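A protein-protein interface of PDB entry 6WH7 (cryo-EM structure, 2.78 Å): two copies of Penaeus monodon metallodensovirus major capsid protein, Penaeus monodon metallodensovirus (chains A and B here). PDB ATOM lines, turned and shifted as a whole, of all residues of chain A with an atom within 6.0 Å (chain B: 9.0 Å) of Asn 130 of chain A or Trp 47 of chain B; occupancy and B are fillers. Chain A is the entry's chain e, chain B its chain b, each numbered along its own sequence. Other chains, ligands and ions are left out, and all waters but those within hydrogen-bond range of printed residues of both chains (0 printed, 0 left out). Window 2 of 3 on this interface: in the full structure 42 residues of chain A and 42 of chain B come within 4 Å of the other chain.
The backbone NH of Thr 50 of chain B sits at hydrogen-bond distance from the side-chain carboxylate of Glu 294 of chain A, at 3.3 Å.
Arg 67 of chain A touches Thr 49 of chain B (NH1 to CB, 3.5 Å).
Ser 129 of chain A touches Trp 47 of chain B (OG to CZ2, 3.0 Å).
OD1 of Asn 130 of chain A touches CE3 of Trp 47 of chain B, at 3.0 Å.
Thr 49 of chain B touches Glu 294 of chain A.
The side-chain amide oxygen of Asn 130 of chain A is in hydrogen-bond range of the side-chain hydroxyl of Ser 129 of chain A, 2.7 Å away.
N of Thr 292 of chain A is in hydrogen-bond range of O of Ser 129 of chain A (2.6 Å).
OE2 of Glu 294 of chain A lies within salt-bridge range of NH1 of Arg 67 of chain A, 3.8 Å away.
The backbone NH (N) of Thr 127 of chain A lies within hydrogen-bond range of the backbone carbonyl oxygen (O) of Glu 294 of chain A (2.6 Å).
Printed residues of chain B that touch a printed residue of chain A: Trp 47, Thr 49 and Thr 50.
Hydrophobic or aromatic side chains of chain B within 4 Å of the printed part of chain A: Trp 47.
Of the 14 printed residues of chain A, 4 touch a printed residue of chain B.
Printed residues of chain A that touch a printed residue of chain B: Arg 67, Ser 129, Asn 130 and Glu 294.
Among the printed residues, no Asp or Glu carboxylate lies within 4 Å of a Lys or Arg side-chain nitrogen of the other chain.
Of the printed residues of chain A, Trp 47 of chain B touches Ser 129 (3.0 Å) and Asn 130 (3.0 Å).
Of chain B, only Trp 47 comes within 4 Å of Ser 129 of chain A.
Of the printed residues of chain B, Glu 294 of chain A touches Thr 49 (3.3 Å) and Thr 50 (3.2 Å).
Printed residues of chain B within 4 Å of Arg 67 of chain A: Thr 49 (3.5 Å).
Printed residues of chain A within 4 Å of Thr 50 of chain B: Glu 294 (3.2 Å).
Printed residues of chain A within 4 Å of Thr 49 of chain B: Arg 67 and Glu 294.
Ile 132 of chain A touches none of the printed residues of chain B.
No position is printed for both chains.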
ATOM      1  N   ARG A  67      15.063 -12.568 -11.191  1.00  0.00           N
ATOM      2  CA  ARG A  67      16.232 -13.418 -11.328  1.00  0.00           C
ATOM      3  C   ARG A  67      16.121 -14.603 -10.388  1.00  0.00           C
ATOM      4  O   ARG A  67      15.594 -14.491  -9.281  1.00  0.00           O
ATOM      5  CB  ARG A  67      17.511 -12.643 -11.063  1.00  0.00           C
ATOM      6  CG  ARG A  67      18.764 -13.455 -11.170  1.00  0.00           C
ATOM      7  CD  ARG A  67      19.977 -12.578 -11.063  1.00  0.00           C
ATOM      8  NE  ARG A  67      20.015 -11.832  -9.817  1.00  0.00           N
ATOM      9  CZ  ARG A  67      19.769 -10.533  -9.733  1.00  0.00           C
ATOM     10  NH1 ARG A  67      19.480  -9.847 -10.823  1.00  0.00           N
ATOM     11  NH2 ARG A  67      19.820  -9.922  -8.564  1.00  0.00           N
ATOM     12  N   THR A 127      16.675 -14.935 -19.906  1.00  0.00           N
ATOM     13  CA  THR A 127      18.087 -15.189 -20.139  1.00  0.00           C
ATOM     14  C   THR A 127      18.532 -16.363 -19.291  1.00  0.00           C
ATOM     15  O   THR A 127      18.289 -16.387 -18.085  1.00  0.00           O
ATOM     16  CB  THR A 127      18.940 -13.967 -19.811  1.00  0.00           C
ATOM     17  OG1 THR A 127      18.551 -12.872 -20.643  1.00  0.00           O
ATOM     18  CG2 THR A 127      20.390 -14.267 -20.061  1.00  0.00           C
ATOM     19  N   LEU A 128      19.164 -17.338 -19.928  1.00  0.00           N
ATOM     20  CA  LEU A 128      19.839 -18.431 -19.247  1.00  0.00           C
ATOM     21  C   LEU A 128      21.319 -18.115 -19.184  1.00  0.00           C
ATOM     22  O   LEU A 128      21.931 -17.806 -20.205  1.00  0.00           O
ATOM     23  CB  LEU A 128      19.606 -19.749 -19.976  1.00  0.00           C
ATOM     24  CG  LEU A 128      18.496 -20.632 -19.438  1.00  0.00           C
ATOM     25  CD1 LEU A 128      17.219 -19.885 -19.334  1.00  0.00           C
ATOM     26  CD2 LEU A 128      18.328 -21.799 -20.374  1.00  0.00           C
ATOM     27  N   SER A 129      21.888 -18.183 -17.992  1.00  0.00           N
ATOM     28  CA  SER A 129      23.221 -17.658 -17.782  1.00  0.00           C
ATOM     29  C   SER A 129      23.986 -18.528 -16.804  1.00  0.00           C
ATOM     30  O   SER A 129      23.408 -19.120 -15.896  1.00  0.00           O
ATOM     31  CB  SER A 129      23.157 -16.231 -17.259  1.00  0.00           C
ATOM     32  OG  SER A 129      24.451 -15.759 -16.989  1.00  0.00           O
ATOM     33  N   ASN A 130      25.301 -18.595 -17.009  1.00  0.00           N
ATOM     34  CA  ASN A 130      26.250 -19.148 -16.048  1.00  0.00           C
ATOM     35  C   ASN A 130      25.917 -20.606 -15.727  1.00  0.00           C
ATOM     36  O   ASN A 130      25.584 -20.979 -14.602  1.00  0.00           O
ATOM     37  CB  ASN A 130      26.284 -18.268 -14.798  1.00  0.00           C
ATOM     38  CG  ASN A 130      26.749 -16.871 -15.108  1.00  0.00           C
ATOM     39  OD1 ASN A 130      26.047 -15.905 -14.850  1.00  0.00           O
ATOM     40  ND2 ASN A 130      27.944 -16.755 -15.657  1.00  0.00           N
ATOM     41  N   LEU A 131      26.044 -21.423 -16.769  1.00  0.00           N
ATOM     42  CA  LEU A 131      25.710 -22.834 -16.673  1.00  0.00           C
ATOM     43  C   LEU A 131      26.751 -23.574 -15.857  1.00  0.00           C
ATOM     44  O   LEU A 131      27.951 -23.410 -16.076  1.00  0.00           O
ATOM     45  CB  LEU A 131      25.609 -23.447 -18.062  1.00  0.00           C
ATOM     46  CG  LEU A 131      25.302 -24.934 -18.114  1.00  0.00           C
ATOM     47  CD1 LEU A 131      23.935 -25.207 -17.556  1.00  0.00           C
ATOM     48  CD2 LEU A 131      25.403 -25.437 -19.504  1.00  0.00           C
ATOM     49  N   ILE A 132      26.289 -24.389 -14.914  1.00  0.00           N
ATOM     50  CA  ILE A 132      27.142 -25.269 -14.127  1.00  0.00           C
ATOM     51  C   ILE A 132      26.627 -26.685 -14.301  1.00  0.00           C
ATOM     52  O   ILE A 132      25.489 -26.984 -13.930  1.00  0.00           O
ATOM     53  CB  ILE A 132      27.172 -24.886 -12.640  1.00  0.00           C
ATOM     54  CG1 ILE A 132      27.826 -23.528 -12.453  1.00  0.00           C
ATOM     55  CG2 ILE A 132      27.921 -25.929 -11.846  1.00  0.00           C
ATOM     56  CD1 ILE A 132      27.665 -22.984 -11.072  1.00  0.00           C
ATOM     57  N   TRP A 211      24.965 -25.935 -25.025  1.00  0.00           N
ATOM     58  CA  TRP A 211      25.403 -24.828 -24.200  1.00  0.00           C
ATOM     59  C   TRP A 211      26.299 -25.378 -23.110  1.00  0.00           C
ATOM     60  O   TRP A 211      25.915 -26.295 -22.384  1.00  0.00           O
ATOM     61  CB  TRP A 211      24.193 -24.066 -23.669  1.00  0.00           C
ATOM     62  CG  TRP A 211      24.477 -22.878 -22.840  1.00  0.00           C
ATOM     63  CD1 TRP A 211      25.184 -21.785 -23.205  1.00  0.00           C
ATOM     64  CD2 TRP A 211      23.865 -22.551 -21.592  1.00  0.00           C
ATOM     65  NE1 TRP A 211      25.159 -20.842 -22.216  1.00  0.00           N
ATOM     66  CE2 TRP A 211      24.338 -21.287 -21.218  1.00  0.00           C
ATOM     67  CE3 TRP A 211      22.990 -23.221 -20.733  1.00  0.00           C
ATOM     68  CZ2 TRP A 211      23.975 -20.684 -20.024  1.00  0.00           C
ATOM     69  CZ3 TRP A 211      22.629 -22.618 -19.558  1.00  0.00           C
ATOM     70  CH2 TRP A 211      23.121 -21.367 -19.207  1.00  0.00           C
ATOM     71  N   ASP A 215      30.189 -20.732 -21.776  1.00  0.00           N
ATOM     72  CA  ASP A 215      29.540 -20.075 -22.893  1.00  0.00           C
ATOM     73  C   ASP A 215      28.787 -18.840 -22.424  1.00  0.00           C
ATOM     74  O   ASP A 215      28.415 -18.704 -21.258  1.00  0.00           O
ATOM     75  CB  ASP A 215      28.576 -21.015 -23.609  1.00  0.00           C
ATOM     76  CG  ASP A 215      29.279 -22.010 -24.492  1.00  0.00           C
ATOM     77  OD1 ASP A 215      30.483 -21.830 -24.750  1.00  0.00           O
ATOM     78  OD2 ASP A 215      28.618 -22.957 -24.957  1.00  0.00           O
ATOM     79  N   ALA A 217      25.673 -16.141 -22.140  1.00  0.00           N
ATOM     80  CA  ALA A 217      24.300 -16.376 -21.730  1.00  0.00           C
ATOM     81  C   ALA A 217      23.396 -16.563 -22.939  1.00  0.00           C
ATOM     82  O   ALA A 217      23.662 -16.055 -24.030  1.00  0.00           O
ATOM     83  CB  ALA A 217      23.797 -15.215 -20.882  1.00  0.00           C
ATOM     84  N   GLN A 290      23.062 -26.372 -13.221  1.00  0.00           N
ATOM     85  CA  GLN A 290      22.632 -25.126 -12.621  1.00  0.00           C
ATOM     86  C   GLN A 290      22.877 -23.998 -13.608  1.00  0.00           C
ATOM     87  O   GLN A 290      23.877 -23.991 -14.324  1.00  0.00           O
ATOM     88  CB  GLN A 290      23.388 -24.777 -11.345  1.00  0.00           C
ATOM     89  CG  GLN A 290      22.715 -23.620 -10.654  1.00  0.00           C
ATOM     90  CD  GLN A 290      23.612 -22.858  -9.751  1.00  0.00           C
ATOM     91  OE1 GLN A 290      24.806 -23.104  -9.701  1.00  0.00           O
ATOM     92  NE2 GLN A 290      23.051 -21.918  -9.030  1.00  0.00           N
ATOM     93  N   PHE A 291      21.974 -23.034 -13.620  1.00  0.00           N
ATOM     94  CA  PHE A 291      22.195 -21.793 -14.339  1.00  0.00           C
ATOM     95  C   PHE A 291      21.360 -20.717 -13.671  1.00  0.00           C
ATOM     96  O   PHE A 291      20.616 -20.978 -12.725  1.00  0.00           O
ATOM     97  CB  PHE A 291      21.867 -21.950 -15.825  1.00  0.00           C
ATOM     98  CG  PHE A 291      20.522 -22.535 -16.085  1.00  0.00           C
ATOM     99  CD1 PHE A 291      19.409 -21.737 -16.192  1.00  0.00           C
ATOM    100  CD2 PHE A 291      20.374 -23.895 -16.208  1.00  0.00           C
ATOM    101  CE1 PHE A 291      18.187 -22.284 -16.419  1.00  0.00           C
ATOM    102  CE2 PHE A 291      19.158 -24.439 -16.437  1.00  0.00           C
ATOM    103  CZ  PHE A 291      18.064 -23.636 -16.548  1.00  0.00           C
ATOM    104  N   THR A 292      21.496 -19.499 -14.167  1.00  0.00           N
ATOM    105  CA  THR A 292      20.751 -18.364 -13.659  1.00  0.00           C
ATOM    106  C   THR A 292      19.641 -18.035 -14.643  1.00  0.00           C
ATOM    107  O   THR A 292      19.884 -17.935 -15.846  1.00  0.00           O
ATOM    108  CB  THR A 292      21.667 -17.160 -13.465  1.00  0.00           C
ATOM    109  OG1 THR A 292      22.725 -17.516 -12.575  1.00  0.00           O
ATOM    110  CG2 THR A 292      20.907 -16.010 -12.873  1.00  0.00           C
ATOM    111  N   GLU A 294      17.172 -15.189 -15.613  1.00  0.00           N
ATOM    112  CA  GLU A 294      16.719 -13.808 -15.559  1.00  0.00           C
ATOM    113  C   GLU A 294      15.624 -13.618 -16.590  1.00  0.00           C
ATOM    114  O   GLU A 294      15.876 -13.724 -17.792  1.00  0.00           O
ATOM    115  CB  GLU A 294      17.861 -12.833 -15.822  1.00  0.00           C
ATOM    116  CG  GLU A 294      18.829 -12.678 -14.691  1.00  0.00           C
ATOM    117  CD  GLU A 294      19.943 -11.722 -15.031  1.00  0.00           C
ATOM    118  OE1 GLU A 294      20.115 -11.416 -16.227  1.00  0.00           O
ATOM    119  OE2 GLU A 294      20.628 -11.250 -14.107  1.00  0.00           O
ATOM    120  N   SER B  45      36.821  -9.775 -17.618  1.00  0.00           N
ATOM    121  CA  SER B  45      35.459  -9.327 -17.371  1.00  0.00           C
ATOM    122  C   SER B  45      34.719 -10.311 -16.480  1.00  0.00           C
ATOM    123  O   SER B  45      34.501 -11.462 -16.855  1.00  0.00           O
ATOM    124  CB  SER B  45      34.706  -9.141 -18.688  1.00  0.00           C
ATOM    125  OG  SER B  45      33.372  -8.720 -18.463  1.00  0.00           O
ATOM    126  N   VAL B  46      34.345  -9.851 -15.294  1.00  0.00           N
ATOM    127  CA  VAL B  46      33.557 -10.657 -14.373  1.00  0.00           C
ATOM    128  C   VAL B  46      32.088 -10.497 -14.732  1.00  0.00           C
ATOM    129  O   VAL B  46      31.606  -9.377 -14.936  1.00  0.00           O
ATOM    130  CB  VAL B  46      33.831 -10.240 -12.920  1.00  0.00           C
ATOM    131  CG1 VAL B  46      32.951 -11.001 -11.972  1.00  0.00           C
ATOM    132  CG2 VAL B  46      35.289 -10.467 -12.584  1.00  0.00           C
ATOM    133  N   TRP B  47      31.375 -11.614 -14.830  1.00  0.00           N
ATOM    134  CA  TRP B  47      29.978 -11.563 -15.223  1.00  0.00           C
ATOM    135  C   TRP B  47      29.143 -10.976 -14.098  1.00  0.00           C
ATOM    136  O   TRP B  47      29.362 -11.273 -12.924  1.00  0.00           O
ATOM    137  CB  TRP B  47      29.461 -12.956 -15.569  1.00  0.00           C
ATOM    138  CG  TRP B  47      28.090 -12.927 -16.149  1.00  0.00           C
ATOM    139  CD1 TRP B  47      27.768 -12.836 -17.464  1.00  0.00           C
ATOM    140  CD2 TRP B  47      26.853 -12.954 -15.434  1.00  0.00           C
ATOM    141  NE1 TRP B  47      26.409 -12.821 -17.619  1.00  0.00           N
ATOM    142  CE2 TRP B  47      25.824 -12.891 -16.385  1.00  0.00           C
ATOM    143  CE3 TRP B  47      26.514 -13.026 -14.083  1.00  0.00           C
ATOM    144  CZ2 TRP B  47      24.484 -12.899 -16.031  1.00  0.00           C
ATOM    145  CZ3 TRP B  47      25.187 -13.037 -13.737  1.00  0.00           C
ATOM    146  CH2 TRP B  47      24.189 -12.978 -14.701  1.00  0.00           C
ATOM    147  N   GLN B  48      28.175 -10.140 -14.458  1.00  0.00           N
ATOM    148  CA  GLN B  48      27.307  -9.564 -13.452  1.00  0.00           C
ATOM    149  C   GLN B  48      25.878  -9.486 -13.964  1.00  0.00           C
ATOM    150  O   GLN B  48      25.615  -9.456 -15.166  1.00  0.00           O
ATOM    151  CB  GLN B  48      27.805  -8.190 -12.997  1.00  0.00           C
ATOM    152  CG  GLN B  48      27.824  -7.134 -14.051  1.00  0.00           C
ATOM    153  CD  GLN B  48      28.386  -5.843 -13.522  1.00  0.00           C
ATOM    154  OE1 GLN B  48      29.095  -5.833 -12.522  1.00  0.00           O
ATOM    155  NE2 GLN B  48      28.066  -4.740 -14.183  1.00  0.00           N
ATOM    156  N   THR B  49      24.957  -9.463 -13.009  1.00  0.00           N
ATOM    157  CA  THR B  49      23.530  -9.505 -13.256  1.00  0.00           C
ATOM    158  C   THR B  49      23.030  -8.177 -13.815  1.00  0.00           C
ATOM    159  O   THR B  49      23.714  -7.153 -13.769  1.00  0.00           O
ATOM    160  CB  THR B  49      22.788  -9.842 -11.971  1.00  0.00           C
ATOM    161  OG1 THR B  49      23.076  -8.848 -10.985  1.00  0.00           O
ATOM    162  CG2 THR B  49      23.234 -11.179 -11.455  1.00  0.00           C
ATOM    163  N   THR B  50      21.823  -8.213 -14.372  1.00  0.00           N
ATOM    164  CA  THR B  50      21.220  -7.014 -14.930  1.00  0.00           C
ATOM    165  C   THR B  50      20.982  -5.969 -13.848  1.00  0.00           C
ATOM    166  O   THR B  50      20.867  -6.270 -12.658  1.00  0.00           O
ATOM    167  CB  THR B  50      19.893  -7.335 -15.611  1.00  0.00           C
ATOM    168  OG1 THR B  50      19.002  -7.931 -14.662  1.00  0.00           O
ATOM    169  CG2 THR B  50      20.102  -8.279 -16.767  1.00  0.00           C
ATOM    170  N   ASP B  51      20.900  -4.720 -14.285  1.00  0.00           N
ATOM    171  CA  ASP B  51      20.686  -3.601 -13.384  1.00  0.00           C
ATOM    172  C   ASP B  51      19.220  -3.513 -12.993  1.00  0.00           C
ATOM    173  O   ASP B  51      18.342  -3.489 -13.858  1.00  0.00           O
ATOM    174  CB  ASP B  51      21.133  -2.307 -14.056  1.00  0.00           C
ATOM    175  CG  ASP B  51      20.975  -1.106 -13.165  1.00  0.00           C
ATOM    176  OD1 ASP B  51      21.699  -1.017 -12.152  1.00  0.00           O
ATOM    177  OD2 ASP B  51      20.132  -0.245 -13.479  1.00  0.00           O
